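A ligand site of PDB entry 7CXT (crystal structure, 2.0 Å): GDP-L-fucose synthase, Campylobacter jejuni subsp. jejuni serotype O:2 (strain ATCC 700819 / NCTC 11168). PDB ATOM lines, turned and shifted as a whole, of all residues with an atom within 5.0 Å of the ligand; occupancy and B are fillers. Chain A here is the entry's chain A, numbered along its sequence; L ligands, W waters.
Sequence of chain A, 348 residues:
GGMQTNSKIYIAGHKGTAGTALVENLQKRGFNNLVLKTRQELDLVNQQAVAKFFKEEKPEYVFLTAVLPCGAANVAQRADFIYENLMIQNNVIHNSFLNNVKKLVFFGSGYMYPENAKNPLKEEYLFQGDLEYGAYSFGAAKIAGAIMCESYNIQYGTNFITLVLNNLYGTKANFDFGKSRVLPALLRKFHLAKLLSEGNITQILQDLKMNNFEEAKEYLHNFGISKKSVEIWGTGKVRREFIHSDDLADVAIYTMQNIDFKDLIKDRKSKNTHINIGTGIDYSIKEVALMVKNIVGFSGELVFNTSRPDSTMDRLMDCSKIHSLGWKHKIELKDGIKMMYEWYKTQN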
ATOM      1  N   GLY A  13      12.329 -25.438   5.205  1.00  0.00           N
ATOM      2  CA  GLY A  13      12.722 -25.887   6.533  1.00  0.00           C
ATOM      3  C   GLY A  13      11.780 -26.906   7.146  1.00  0.00           C
ATOM      4  O   GLY A  13      11.504 -26.851   8.356  1.00  0.00           O
ATOM      5  N   HIS A  14      11.287 -27.846   6.358  1.00  0.00           N
ATOM      6  CA  HIS A  14      10.136 -28.646   6.753  1.00  0.00           C
ATOM      7  C   HIS A  14      10.445 -29.663   7.860  1.00  0.00           C
ATOM      8  O   HIS A  14       9.497 -30.255   8.407  1.00  0.00           O
ATOM      9  CB  HIS A  14       9.600 -29.383   5.546  1.00  0.00           C
ATOM     10  CG  HIS A  14      10.516 -30.466   5.052  1.00  0.00           C
ATOM     11  ND1 HIS A  14      11.697 -30.202   4.407  1.00  0.00           N
ATOM     12  CD2 HIS A  14      10.423 -31.820   5.137  1.00  0.00           C
ATOM     13  CE1 HIS A  14      12.296 -31.340   4.097  1.00  0.00           C
ATOM     14  NE2 HIS A  14      11.541 -32.337   4.526  1.00  0.00           N
ATOM     15  N   LYS A  15      11.716 -29.931   8.169  1.00  0.00           N
ATOM     16  CA  LYS A  15      12.059 -30.868   9.240  1.00  0.00           C
ATOM     17  C   LYS A  15      12.082 -30.228  10.629  1.00  0.00           C
ATOM     18  O   LYS A  15      12.143 -30.971  11.623  1.00  0.00           O
ATOM     19  CB  LYS A  15      13.414 -31.532   8.935  1.00  0.00           C
ATOM     20  CG  LYS A  15      13.299 -32.444   7.708  1.00  0.00           C
ATOM     21  CD  LYS A  15      13.895 -33.825   7.937  1.00  0.00           C
ATOM     22  CE  LYS A  15      15.391 -33.842   7.608  1.00  0.00           C
ATOM     23  NZ  LYS A  15      15.877 -35.194   7.189  1.00  0.00           N
ATOM     24  N   GLY A  16      12.005 -28.901  10.741  1.00  0.00           N
ATOM     25  CA  GLY A  16      12.033 -28.253  12.032  1.00  0.00           C
ATOM     26  C   GLY A  16      10.701 -28.364  12.753  1.00  0.00           C
ATOM     27  O   GLY A  16       9.751 -28.979  12.275  1.00  0.00           O
ATOM     28  N   THR A  17      10.638 -27.775  13.949  1.00  0.00           N
ATOM     29  CA  THR A  17       9.424 -27.886  14.774  1.00  0.00           C
ATOM     30  C   THR A  17       8.207 -27.292  14.065  1.00  0.00           C
ATOM     31  O   THR A  17       7.185 -27.959  13.901  1.00  0.00           O
ATOM     32  CB  THR A  17       9.638 -27.219  16.125  1.00  0.00           C
ATOM     33  OG1 THR A  17      10.759 -27.840  16.768  1.00  0.00           O
ATOM     34  CG2 THR A  17       8.385 -27.379  16.989  1.00  0.00           C
ATOM     35  N   ALA A  18       8.292 -26.022  13.631  1.00  0.00           N
ATOM     36  CA  ALA A  18       7.160 -25.442  12.904  1.00  0.00           C
ATOM     37  C   ALA A  18       6.926 -26.154  11.584  1.00  0.00           C
ATOM     38  O   ALA A  18       5.764 -26.395  11.197  1.00  0.00           O
ATOM     39  CB  ALA A  18       7.400 -23.942  12.648  1.00  0.00           C
ATOM     40  N   GLY A  19       8.005 -26.553  10.897  1.00  0.00           N
ATOM     41  CA  GLY A  19       7.836 -27.136   9.579  1.00  0.00           C
ATOM     42  C   GLY A  19       7.152 -28.481   9.616  1.00  0.00           C
ATOM     43  O   GLY A  19       6.289 -28.765   8.783  1.00  0.00           O
ATOM     44  N   ARG A  39      17.917 -29.712   4.104  1.00  0.00           N
ATOM     45  CA  ARG A  39      19.061 -28.819   4.008  1.00  0.00           C
ATOM     46  C   ARG A  39      20.103 -29.375   3.045  1.00  0.00           C
ATOM     47  O   ARG A  39      20.681 -28.645   2.241  1.00  0.00           O
ATOM     48  CB  ARG A  39      19.673 -28.633   5.398  1.00  0.00           C
ATOM     49  CG  ARG A  39      20.883 -27.713   5.447  1.00  0.00           C
ATOM     50  CD  ARG A  39      21.376 -27.602   6.887  1.00  0.00           C
ATOM     51  NE  ARG A  39      22.050 -26.316   7.125  1.00  0.00           N
ATOM     52  CZ  ARG A  39      21.743 -25.478   8.112  1.00  0.00           C
ATOM     53  NH1 ARG A  39      20.778 -25.768   8.977  1.00  0.00           N
ATOM     54  NH2 ARG A  39      22.420 -24.346   8.224  1.00  0.00           N
ATOM     55  N   GLN A  40      20.309 -30.698   3.082  1.00  0.00           N
ATOM     56  CA  GLN A  40      21.314 -31.301   2.207  1.00  0.00           C
ATOM     57  C   GLN A  40      20.921 -31.222   0.751  1.00  0.00           C
ATOM     58  O   GLN A  40      21.799 -31.198  -0.125  1.00  0.00           O
ATOM     59  CB  GLN A  40      21.575 -32.749   2.625  1.00  0.00           C
ATOM     60  CG  GLN A  40      22.332 -32.881   3.948  1.00  0.00           C
ATOM     61  CD  GLN A  40      21.524 -32.447   5.154  1.00  0.00           C
ATOM     62  OE1 GLN A  40      20.288 -32.606   5.200  1.00  0.00           O
ATOM     63  NE2 GLN A  40      22.209 -31.903   6.147  1.00  0.00           N
ATOM     64  N   LEU A  42      19.073 -28.626  -0.488  1.00  0.00           N
ATOM     65  CA  LEU A  42      18.886 -27.216  -0.842  1.00  0.00           C
ATOM     66  C   LEU A  42      19.362 -26.352   0.317  1.00  0.00           C
ATOM     67  O   LEU A  42      18.737 -26.298   1.372  1.00  0.00           O
ATOM     68  CB  LEU A  42      17.417 -26.927  -1.176  1.00  0.00           C
ATOM     69  CG  LEU A  42      16.959 -25.467  -1.255  1.00  0.00           C
ATOM     70  CD1 LEU A  42      17.722 -24.682  -2.327  1.00  0.00           C
ATOM     71  CD2 LEU A  42      15.426 -25.359  -1.493  1.00  0.00           C
ATOM     72  N   ASP A  43      20.496 -25.683   0.135  1.00  0.00           N
ATOM     73  CA  ASP A  43      21.021 -24.766   1.141  1.00  0.00           C
ATOM     74  C   ASP A  43      20.403 -23.386   0.888  1.00  0.00           C
ATOM     75  O   ASP A  43      20.799 -22.699  -0.050  1.00  0.00           O
ATOM     76  CB  ASP A  43      22.554 -24.718   1.075  1.00  0.00           C
ATOM     77  CG  ASP A  43      23.172 -23.749   2.084  1.00  0.00           C
ATOM     78  OD1 ASP A  43      22.432 -23.065   2.816  1.00  0.00           O
ATOM     79  OD2 ASP A  43      24.412 -23.678   2.123  1.00  0.00           O
ATOM     80  N   LEU A  44      19.458 -22.986   1.755  1.00  0.00           N
ATOM     81  CA  LEU A  44      18.707 -21.761   1.539  1.00  0.00           C
ATOM     82  C   LEU A  44      19.548 -20.498   1.647  1.00  0.00           C
ATOM     83  O   LEU A  44      19.042 -19.421   1.315  1.00  0.00           O
ATOM     84  CB  LEU A  44      17.540 -21.693   2.532  1.00  0.00           C
ATOM     85  CG  LEU A  44      16.483 -22.747   2.254  1.00  0.00           C
ATOM     86  CD1 LEU A  44      15.486 -22.743   3.405  1.00  0.00           C
ATOM     87  CD2 LEU A  44      15.814 -22.505   0.902  1.00  0.00           C
ATOM     88  N   VAL A  45      20.774 -20.583   2.169  1.00  0.00           N
ATOM     89  CA  VAL A  45      21.675 -19.438   2.145  1.00  0.00           C
ATOM     90  C   VAL A  45      22.252 -19.218   0.740  1.00  0.00           C
ATOM     91  O   VAL A  45      22.704 -18.119   0.405  1.00  0.00           O
ATOM     92  CB  VAL A  45      22.789 -19.662   3.188  1.00  0.00           C
ATOM     93  CG1 VAL A  45      23.970 -18.648   3.035  1.00  0.00           C
ATOM     94  CG2 VAL A  45      22.195 -19.597   4.585  1.00  0.00           C
ATOM     95  N   LEU A  64       7.700 -20.133   5.136  1.00  0.00           N
ATOM     96  CA  LEU A  64       9.158 -19.985   5.326  1.00  0.00           C
ATOM     97  C   LEU A  64       9.494 -20.181   6.804  1.00  0.00           C
ATOM     98  O   LEU A  64       9.521 -19.221   7.574  1.00  0.00           O
ATOM     99  CB  LEU A  64       9.643 -18.612   4.827  1.00  0.00           C
ATOM    100  CG  LEU A  64      11.090 -18.180   5.115  1.00  0.00           C
ATOM    101  CD1 LEU A  64      12.131 -19.227   4.637  1.00  0.00           C
ATOM    102  CD2 LEU A  64      11.389 -16.837   4.478  1.00  0.00           C
ATOM    103  N   THR A  65       9.779 -21.422   7.195  1.00  0.00           N
ATOM    104  CA  THR A  65      10.114 -21.712   8.585  1.00  0.00           C
ATOM    105  C   THR A  65      11.607 -21.833   8.852  1.00  0.00           C
ATOM    106  O   THR A  65      11.993 -21.858  10.017  1.00  0.00           O
ATOM    107  CB  THR A  65       9.413 -23.003   9.070  1.00  0.00           C
ATOM    108  OG1 THR A  65      10.124 -24.158   8.591  1.00  0.00           O
ATOM    109  CG2 THR A  65       7.975 -23.064   8.587  1.00  0.00           C
ATOM    110  N   ALA A  66      12.442 -21.928   7.818  1.00  0.00           N
ATOM    111  CA  ALA A  66      13.864 -22.184   8.046  1.00  0.00           C
ATOM    112  C   ALA A  66      14.557 -20.993   8.700  1.00  0.00           C
ATOM    113  O   ALA A  66      14.362 -19.842   8.293  1.00  0.00           O
ATOM    114  CB  ALA A  66      14.556 -22.532   6.734  1.00  0.00           C
ATOM    115  N   VAL A  67      15.428 -21.280   9.661  1.00  0.00           N
ATOM    116  CA  VAL A  67      16.059 -20.240  10.472  1.00  0.00           C
ATOM    117  C   VAL A  67      17.327 -20.827  11.057  1.00  0.00           C
ATOM    118  O   VAL A  67      17.423 -22.036  11.264  1.00  0.00           O
ATOM    119  CB  VAL A  67      15.088 -19.761  11.595  1.00  0.00           C
ATOM    120  CG1 VAL A  67      14.764 -20.931  12.550  1.00  0.00           C
ATOM    121  CG2 VAL A  67      15.664 -18.595  12.416  1.00  0.00           C
ATOM    122  N   LEU A  68      18.309 -19.959  11.338  1.00  0.00           N
ATOM    123  CA  LEU A  68      19.346 -20.306  12.289  1.00  0.00           C
ATOM    124  C   LEU A  68      18.967 -19.604  13.579  1.00  0.00           C
ATOM    125  O   LEU A  68      19.047 -18.368  13.650  1.00  0.00           O
ATOM    126  CB  LEU A  68      20.721 -19.845  11.797  1.00  0.00           C
ATOM    127  CG  LEU A  68      21.832 -19.758  12.847  1.00  0.00           C
ATOM    128  CD1 LEU A  68      22.085 -21.123  13.513  1.00  0.00           C
ATOM    129  CD2 LEU A  68      23.124 -19.236  12.233  1.00  0.00           C
ATOM    130  N   PRO A  69      18.560 -20.332  14.617  1.00  0.00           N
ATOM    131  CA  PRO A  69      17.864 -19.666  15.732  1.00  0.00           C
ATOM    132  C   PRO A  69      18.840 -19.295  16.829  1.00  0.00           C
ATOM    133  O   PRO A  69      19.862 -19.968  17.018  1.00  0.00           O
ATOM    134  CB  PRO A  69      16.852 -20.727  16.184  1.00  0.00           C
ATOM    135  CG  PRO A  69      17.569 -22.030  15.934  1.00  0.00           C
ATOM    136  CD  PRO A  69      18.546 -21.800  14.769  1.00  0.00           C
ATOM    137  N   ILE A  88      18.719 -16.402   3.967  1.00  0.00           N
ATOM    138  CA  ILE A  88      17.533 -17.237   3.816  1.00  0.00           C
ATOM    139  C   ILE A  88      16.310 -16.382   3.499  1.00  0.00           C
ATOM    140  O   ILE A  88      15.565 -16.649   2.544  1.00  0.00           O
ATOM    141  CB  ILE A  88      17.298 -18.073   5.089  1.00  0.00           C
ATOM    142  CG1 ILE A  88      18.481 -19.016   5.356  1.00  0.00           C
ATOM    143  CG2 ILE A  88      15.975 -18.831   5.013  1.00  0.00           C
ATOM    144  CD1 ILE A  88      18.309 -19.746   6.686  1.00  0.00           C
ATOM    145  N   PHE A 106       5.871 -15.736   6.513  1.00  0.00           N
ATOM    146  CA  PHE A 106       7.169 -15.693   7.144  1.00  0.00           C
ATOM    147  C   PHE A 106       6.967 -15.619   8.650  1.00  0.00           C
ATOM    148  O   PHE A 106       6.015 -14.988   9.114  1.00  0.00           O
ATOM    149  CB  PHE A 106       7.982 -14.484   6.621  1.00  0.00           C
ATOM    150  CG  PHE A 106       9.223 -14.197   7.397  1.00  0.00           C
ATOM    151  CD1 PHE A 106      10.207 -15.177   7.543  1.00  0.00           C
ATOM    152  CD2 PHE A 106       9.422 -12.959   7.987  1.00  0.00           C
ATOM    153  CE1 PHE A 106      11.354 -14.916   8.276  1.00  0.00           C
ATOM    154  CE2 PHE A 106      10.569 -12.680   8.703  1.00  0.00           C
ATOM    155  CZ  PHE A 106      11.556 -13.664   8.833  1.00  0.00           C
ATOM    156  N   PHE A 107       7.832 -16.274   9.401  1.00  0.00           N
ATOM    157  CA  PHE A 107       7.656 -16.288  10.856  1.00  0.00           C
ATOM    158  C   PHE A 107       8.687 -15.377  11.507  1.00  0.00           C
ATOM    159  O   PHE A 107       9.891 -15.509  11.274  1.00  0.00           O
ATOM    160  CB  PHE A 107       7.732 -17.708  11.393  1.00  0.00           C
ATOM    161  CG  PHE A 107       6.593 -18.560  10.939  1.00  0.00           C
ATOM    162  CD1 PHE A 107       5.401 -18.568  11.646  1.00  0.00           C
ATOM    163  CD2 PHE A 107       6.688 -19.292   9.775  1.00  0.00           C
ATOM    164  CE1 PHE A 107       4.320 -19.338  11.204  1.00  0.00           C
ATOM    165  CE2 PHE A 107       5.621 -20.064   9.338  1.00  0.00           C
ATOM    166  CZ  PHE A 107       4.434 -20.076  10.052  1.00  0.00           C
ATOM    167  N   GLY A 108       8.178 -14.414  12.294  1.00  0.00           N
ATOM    168  CA  GLY A 108       9.024 -13.512  13.047  1.00  0.00           C
ATOM    169  C   GLY A 108       9.294 -14.031  14.441  1.00  0.00           C
ATOM    170  O   GLY A 108       8.849 -15.095  14.848  1.00  0.00           O
ATOM    171  N   SER A 109       9.994 -13.211  15.209  1.00  0.00           N
ATOM    172  CA  SER A 109      10.391 -13.571  16.559  1.00  0.00           C
ATOM    173  C   SER A 109      10.170 -12.396  17.488  1.00  0.00           C
ATOM    174  O   SER A 109      10.342 -11.248  17.088  1.00  0.00           O
ATOM    175  CB  SER A 109      11.886 -13.976  16.622  1.00  0.00           C
ATOM    176  OG  SER A 109      12.331 -14.056  17.975  1.00  0.00           O
ATOM    177  N   GLY A 110       9.831 -12.706  18.743  1.00  0.00           N
ATOM    178  CA  GLY A 110       9.684 -11.668  19.744  1.00  0.00           C
ATOM    179  C   GLY A 110      10.963 -10.910  20.030  1.00  0.00           C
ATOM    180  O   GLY A 110      10.921  -9.807  20.581  1.00  0.00           O
ATOM    181  N   PHE A 138      20.289 -11.128  15.737  1.00  0.00           N
ATOM    182  CA  PHE A 138      19.187 -11.998  15.328  1.00  0.00           C
ATOM    183  C   PHE A 138      17.897 -11.217  15.191  1.00  0.00           C
ATOM    184  O   PHE A 138      17.168 -11.363  14.204  1.00  0.00           O
ATOM    185  CB  PHE A 138      19.012 -13.130  16.348  1.00  0.00           C
ATOM    186  CG  PHE A 138      17.859 -14.063  16.040  1.00  0.00           C
ATOM    187  CD1 PHE A 138      18.008 -15.089  15.117  1.00  0.00           C
ATOM    188  CD2 PHE A 138      16.635 -13.929  16.714  1.00  0.00           C
ATOM    189  CE1 PHE A 138      16.941 -15.971  14.842  1.00  0.00           C
ATOM    190  CE2 PHE A 138      15.563 -14.788  16.439  1.00  0.00           C
ATOM    191  CZ  PHE A 138      15.711 -15.806  15.495  1.00  0.00           C
ATOM    192  N   LYS A 142      15.445 -10.416  11.873  1.00  0.00           N
ATOM    193  CA  LYS A 142      14.006 -10.671  11.837  1.00  0.00           C
ATOM    194  C   LYS A 142      13.234  -9.400  11.481  1.00  0.00           C
ATOM    195  O   LYS A 142      12.220  -9.467  10.775  1.00  0.00           O
ATOM    196  CB  LYS A 142      13.519 -11.221  13.177  1.00  0.00           C
ATOM    197  CG  LYS A 142      13.829 -12.691  13.387  1.00  0.00           C
ATOM    198  CD  LYS A 142      13.102 -13.564  12.381  1.00  0.00           C
ATOM    199  CE  LYS A 142      13.435 -15.033  12.615  1.00  0.00           C
ATOM    200  NZ  LYS A 142      12.851 -15.950  11.583  1.00  0.00           N
ATOM    201  N   LEU A 165       6.052 -14.724  16.683  1.00  0.00           N
ATOM    202  CA  LEU A 165       5.752 -15.550  17.852  1.00  0.00           C
ATOM    203  C   LEU A 165       6.920 -15.520  18.833  1.00  0.00           C
ATOM    204  O   LEU A 165       8.040 -15.120  18.488  1.00  0.00           O
ATOM    205  CB  LEU A 165       5.453 -17.006  17.475  1.00  0.00           C
ATOM    206  CG  LEU A 165       6.639 -17.733  16.824  1.00  0.00           C
ATOM    207  CD1 LEU A 165       6.631 -19.183  17.249  1.00  0.00           C
ATOM    208  CD2 LEU A 165       6.571 -17.618  15.307  1.00  0.00           C
ATOM    209  N   ASN A 166       6.636 -15.956  20.079  1.00  0.00           N
ATOM    210  CA  ASN A 166       7.654 -15.976  21.126  1.00  0.00           C
ATOM    211  C   ASN A 166       8.312 -17.335  21.328  1.00  0.00           C
ATOM    212  O   ASN A 166       9.439 -17.535  20.867  1.00  0.00           O
ATOM    213  CB  ASN A 166       7.077 -15.457  22.443  1.00  0.00           C
ATOM    214  CG  ASN A 166       7.068 -13.943  22.494  1.00  0.00           C
ATOM    215  OD1 ASN A 166       8.036 -13.298  22.055  1.00  0.00           O
ATOM    216  ND2 ASN A 166       5.973 -13.360  22.972  1.00  0.00           N
ATOM    217  N   ASN A 167       7.693 -18.264  22.038  1.00  0.00           N
ATOM    218  CA  ASN A 167       8.266 -19.590  22.265  1.00  0.00           C
ATOM    219  C   ASN A 167       7.392 -20.636  21.603  1.00  0.00           C
ATOM    220  O   ASN A 167       6.175 -20.650  21.796  1.00  0.00           O
ATOM    221  CB  ASN A 167       8.398 -19.930  23.752  1.00  0.00           C
ATOM    222  CG  ASN A 167       9.355 -19.019  24.482  1.00  0.00           C
ATOM    223  OD1 ASN A 167       8.937 -18.062  25.152  1.00  0.00           O
ATOM    224  ND2 ASN A 167      10.634 -19.306  24.363  1.00  0.00           N
ATOM    225  N   LEU A 168       8.022 -21.523  20.840  1.00  0.00           N
ATOM    226  CA  LEU A 168       7.346 -22.610  20.170  1.00  0.00           C
ATOM    227  C   LEU A 168       7.555 -23.918  20.933  1.00  0.00           C
ATOM    228  O   LEU A 168       8.604 -24.149  21.520  1.00  0.00           O
ATOM    229  CB  LEU A 168       7.872 -22.767  18.737  1.00  0.00           C
ATOM    230  CG  LEU A 168       6.997 -23.079  17.521  1.00  0.00           C
ATOM    231  CD1 LEU A 168       7.786 -23.923  16.524  1.00  0.00           C
ATOM    232  CD2 LEU A 168       5.655 -23.701  17.853  1.00  0.00           C
ATOM    233  N   ASN A 174      11.857 -30.355  18.679  1.00  0.00           N
ATOM    234  CA  ASN A 174      13.280 -30.656  18.778  1.00  0.00           C
ATOM    235  C   ASN A 174      13.651 -30.689  20.253  1.00  0.00           C
ATOM    236  O   ASN A 174      13.795 -29.657  20.900  1.00  0.00           O
ATOM    237  CB  ASN A 174      14.080 -29.593  18.007  1.00  0.00           C
ATOM    238  CG  ASN A 174      15.576 -29.886  17.981  1.00  0.00           C
ATOM    239  OD1 ASN A 174      16.172 -30.267  18.988  1.00  0.00           O
ATOM    240  ND2 ASN A 174      16.200 -29.672  16.828  1.00  0.00           N
ATOM    241  N   ARG A 181      15.595 -25.556  23.154  1.00  0.00           N
ATOM    242  CA  ARG A 181      14.315 -24.855  23.211  1.00  0.00           C
ATOM    243  C   ARG A 181      13.669 -25.050  24.580  1.00  0.00           C
ATOM    244  O   ARG A 181      13.706 -26.148  25.148  1.00  0.00           O
ATOM    245  CB  ARG A 181      13.397 -25.310  22.082  1.00  0.00           C
ATOM    246  CG  ARG A 181      13.521 -24.409  20.862  1.00  0.00           C
ATOM    247  CD  ARG A 181      12.434 -24.633  19.828  1.00  0.00           C
ATOM    248  NE  ARG A 181      12.745 -25.733  18.928  1.00  0.00           N
ATOM    249  CZ  ARG A 181      13.488 -25.621  17.836  1.00  0.00           C
ATOM    250  NH1 ARG A 181      13.721 -26.679  17.071  1.00  0.00           N
ATOM    251  NH2 ARG A 181      14.006 -24.447  17.506  1.00  0.00           N
HETATM  252  P1  LIG L   1      13.876 -25.079  13.831  1.00  0.00           P
HETATM  253  O1  LIG L   1      15.212 -24.527  14.171  1.00  0.00           O
HETATM  254  O2  LIG L   1      13.186 -26.059  14.744  1.00  0.00           O
HETATM  255  O3  LIG L   1      13.964 -25.803  12.356  1.00  0.00           O
HETATM  256  C1  LIG L   1      14.535 -24.869  11.505  1.00  0.00           C
HETATM  257  C2  LIG L   1      14.702 -25.578  10.150  1.00  0.00           C
HETATM  258  O4  LIG L   1      15.424 -24.760   9.238  1.00  0.00           O
HETATM  259  C3  LIG L   1      15.489 -26.895  10.381  1.00  0.00           C
HETATM  260  O5  LIG L   1      14.836 -27.970   9.764  1.00  0.00           O
HETATM  261  C4  LIG L   1      16.820 -26.591   9.642  1.00  0.00           C
HETATM  262  O6  LIG L   1      17.324 -27.625   9.000  1.00  0.00           O
HETATM  263  C5  LIG L   1      16.315 -25.598   8.565  1.00  0.00           C
HETATM  264  N1  LIG L   1      17.405 -24.791   8.049  1.00  0.00           N
HETATM  265  C6  LIG L   1      18.249 -23.892   8.753  1.00  0.00           C
HETATM  266  N2  LIG L   1      19.151 -23.311   7.970  1.00  0.00           N
HETATM  267  C7  LIG L   1      18.898 -23.870   6.674  1.00  0.00           C
HETATM  268  C8  LIG L   1      19.502 -23.682   5.424  1.00  0.00           C
HETATM  269  N3  LIG L   1      20.572 -22.816   5.238  1.00  0.00           N
HETATM  270  N4  LIG L   1      19.048 -24.324   4.331  1.00  0.00           N
HETATM  271  C9  LIG L   1      17.996 -25.186   4.534  1.00  0.00           C
HETATM  272  N5  LIG L   1      17.318 -25.476   5.637  1.00  0.00           N
HETATM  273  C10 LIG L   1      17.807 -24.789   6.728  1.00  0.00           C
HETATM  274  O7  LIG L   1      13.007 -23.698  13.576  1.00  0.00           O
HETATM  275  P2  LIG L   1      11.588 -23.676  14.340  1.00  0.00           P
HETATM  276  O8  LIG L   1      11.815 -23.603  15.795  1.00  0.00           O
HETATM  277  O9  LIG L   1      10.463 -24.492  13.721  1.00  0.00           O
HETATM  278  O10 LIG L   1      11.030 -22.037  14.061  1.00  0.00           O
HETATM  279  C11 LIG L   1      10.599 -21.856  12.778  1.00  0.00           C
HETATM  280  C12 LIG L   1      10.260 -20.377  12.626  1.00  0.00           C
HETATM  281  O11 LIG L   1       9.627 -19.909  13.856  1.00  0.00           O
HETATM  282  C13 LIG L   1      11.596 -19.549  12.504  1.00  0.00           C
HETATM  283  O12 LIG L   1      11.369 -18.466  11.683  1.00  0.00           O
HETATM  284  C14 LIG L   1      11.840 -19.084  13.950  1.00  0.00           C
HETATM  285  O13 LIG L   1      12.555 -17.876  14.035  1.00  0.00           O
HETATM  286  C15 LIG L   1      10.380 -18.810  14.364  1.00  0.00           C
HETATM  287  N6  LIG L   1      10.298 -18.781  15.819  1.00  0.00           N
HETATM  288  C16 LIG L   1      10.425 -19.932  16.596  1.00  0.00           C
HETATM  289  C17 LIG L   1      10.631 -19.811  17.960  1.00  0.00           C
HETATM  290  C18 LIG L   1      10.792 -21.005  18.786  1.00  0.00           C
HETATM  291  O14 LIG L   1      10.789 -20.996  20.028  1.00  0.00           O
HETATM  292  N7  LIG L   1      10.967 -22.229  18.133  1.00  0.00           N
HETATM  293  C19 LIG L   1      10.724 -18.493  18.620  1.00  0.00           C
HETATM  294  C20 LIG L   1      10.299 -17.390  17.750  1.00  0.00           C
HETATM  295  C21 LIG L   1      10.117 -17.554  16.439  1.00  0.00           C
HETATM  296  P3  LIG L   1      18.484 -28.660   9.941  1.00  0.00           P
HETATM  297  O15 LIG L   1      17.519 -29.226  10.925  1.00  0.00           O
HETATM  298  O16 LIG L   1      18.957 -29.567   8.806  1.00  0.00           O
HETATM  299  O17 LIG L   1      19.420 -27.582  10.421  1.00  0.00           O
HETATM  300  O   HOH W   1      11.648 -18.326   9.131  1.00  0.00           O
HETATM  301  O   HOH W   2      16.913 -30.564   6.891  1.00  0.00           O
HETATM  302  O   HOH W   3      24.052 -22.995   5.329  1.00  0.00           O
HETATM  303  O   HOH W   4      19.280 -24.353  12.061  1.00  0.00           O
HETATM  304  O   HOH W   5      14.724 -28.175  14.974  1.00  0.00           O
HETATM  305  O   HOH W   6      13.788 -18.900  16.371  1.00  0.00           O
HETATM  306  O   HOH W   7      21.779 -21.775   7.518  1.00  0.00           O
HETATM  307  O   HOH W   8      15.152 -27.418   5.180  1.00  0.00           O
HETATM  308  O   HOH W   9      14.522 -29.236   6.975  1.00  0.00           O
HETATM  309  O   HOH W  10      11.540 -21.595  23.146  1.00  0.00           O
HETATM  310  O   HOH W  11      10.723 -25.669  11.165  1.00  0.00           O
HETATM  311  O   HOH W  12      13.651 -21.611  16.707  1.00  0.00           O
HETATM  312  O   HOH W  13      12.740 -19.193  21.323  1.00  0.00           O
HETATM  313  O   HOH W  14      16.117 -26.827   2.136  1.00  0.00           O
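OG1 of Thr 17 lies within hydrogen-bond range of NH1 of Arg 181.
The backbone carbonyl oxygen (O) of Phe 107 lies within hydrogen-bond range of the side-chain amino group (NZ) of Lys 142 (3.0 Å).
N of Val 45 is in hydrogen-bond range of OD1 of Asp 43 (3.1 Å).
The side-chain hydroxyl of Thr 65 is in hydrogen-bond range of the backbone carbonyl oxygen of Gly 13 (3.0 Å).
N of Asn 174 sits at hydrogen-bond distance from OG1 of Thr 17 (3.3 Å).
The backbone NH (N) of Leu 165 sits at hydrogen-bond distance from the backbone carbonyl oxygen (O) of Gly 108 (3.4 Å).
The backbone carbonyl oxygen (O) of Leu 165 is in hydrogen-bond range of the backbone NH (N) of Gly 110.
The guanidinium group of Arg 181 lies within salt-bridge range of an oxygen (O2) of the ligand (2.5 Å).
The backbone NH (N) of Ala 18 sits at hydrogen-bond distance from an oxygen (O9) of the ligand (2.7 Å).
The guanidinium group of Arg 39 is in salt-bridge range of an oxygen (O17) of the ligand, 2.7 Å away.
An oxygen (O12) of the ligand sits at hydrogen-bond distance from the side-chain amino group (NZ) of Lys 142, at 2.9 Å.
The backbone NH (N) of Leu 44 lies within hydrogen-bond range of a nitrogen (N4) of the ligand (2.9 Å).
O14 of the ligand is in hydrogen-bond range of N of Leu 168.
The side-chain carboxylate (OD1) of Asp 43 is in hydrogen-bond range of a nitrogen (N3) of the ligand.
N of Gly 16 lies within hydrogen-bond range of O5 of the ligand (3.1 Å).
N of Thr 17 sits at hydrogen-bond distance from O2 of the ligand (3.2 Å).
The backbone carbonyl oxygen (O) of Phe 107 is in hydrogen-bond range of an oxygen (O12) of the ligand (3.3 Å).
Water W1 lies within hydrogen-bond range of O12 of the ligand, O of Leu 64 and O of Ala 66.
Water W5 lies within hydrogen-bond range of O2 of the ligand (2.6 Å), NH1 of Arg 181 (2.8 Å) and ND2 of Asn 174 (2.8 Å).
Water W7 bridges the guanidinium group (NH2) of Arg 39 (2.7 Å) and a nitrogen (N3) of the ligand (2.8 Å).
Water W8 bridges N5 of the ligand and N of Gly 13.
Water W2 bridges O16 of the ligand (3.0 Å) and N of Arg 39 (3.1 Å).
Water W9 lies within hydrogen-bond range of O5 of the ligand (3.1 Å) and N of Lys 15 (3.1 Å).
Merely in contact with the ligand: Asn 166, Thr 65, Gly 108, Val 67, Ala 66, Leu 165, Leu 42, Asn 167, Val 45, Lys 15, Gly 13, Pro 69, Ile 88 and Ser 109.
Hydrophobic or aromatic side chains that line the ligand: Ala 18, Leu 44, Val 45, Ala 66, Val 67, Pro 69, Ile 88, Phe 107, Leu 165 and Leu 168.
24 residues have an atom within 4 Å of the ligand: Gly 13, Lys 15, Gly 16, Thr 17, Ala 18, Arg 39, Leu 42, Asp 43, Leu 44, Val 45, Thr 65, Ala 66, Val 67, Pro 69, Ile 88, Phe 107, Gly 108, Ser 109, Lys 142, Leu 165, Asn 166, Asn 167, Leu 168 and Arg 181.
The nearest printed residue that does not touch the ligand is Phe 138 (4.05 Å).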
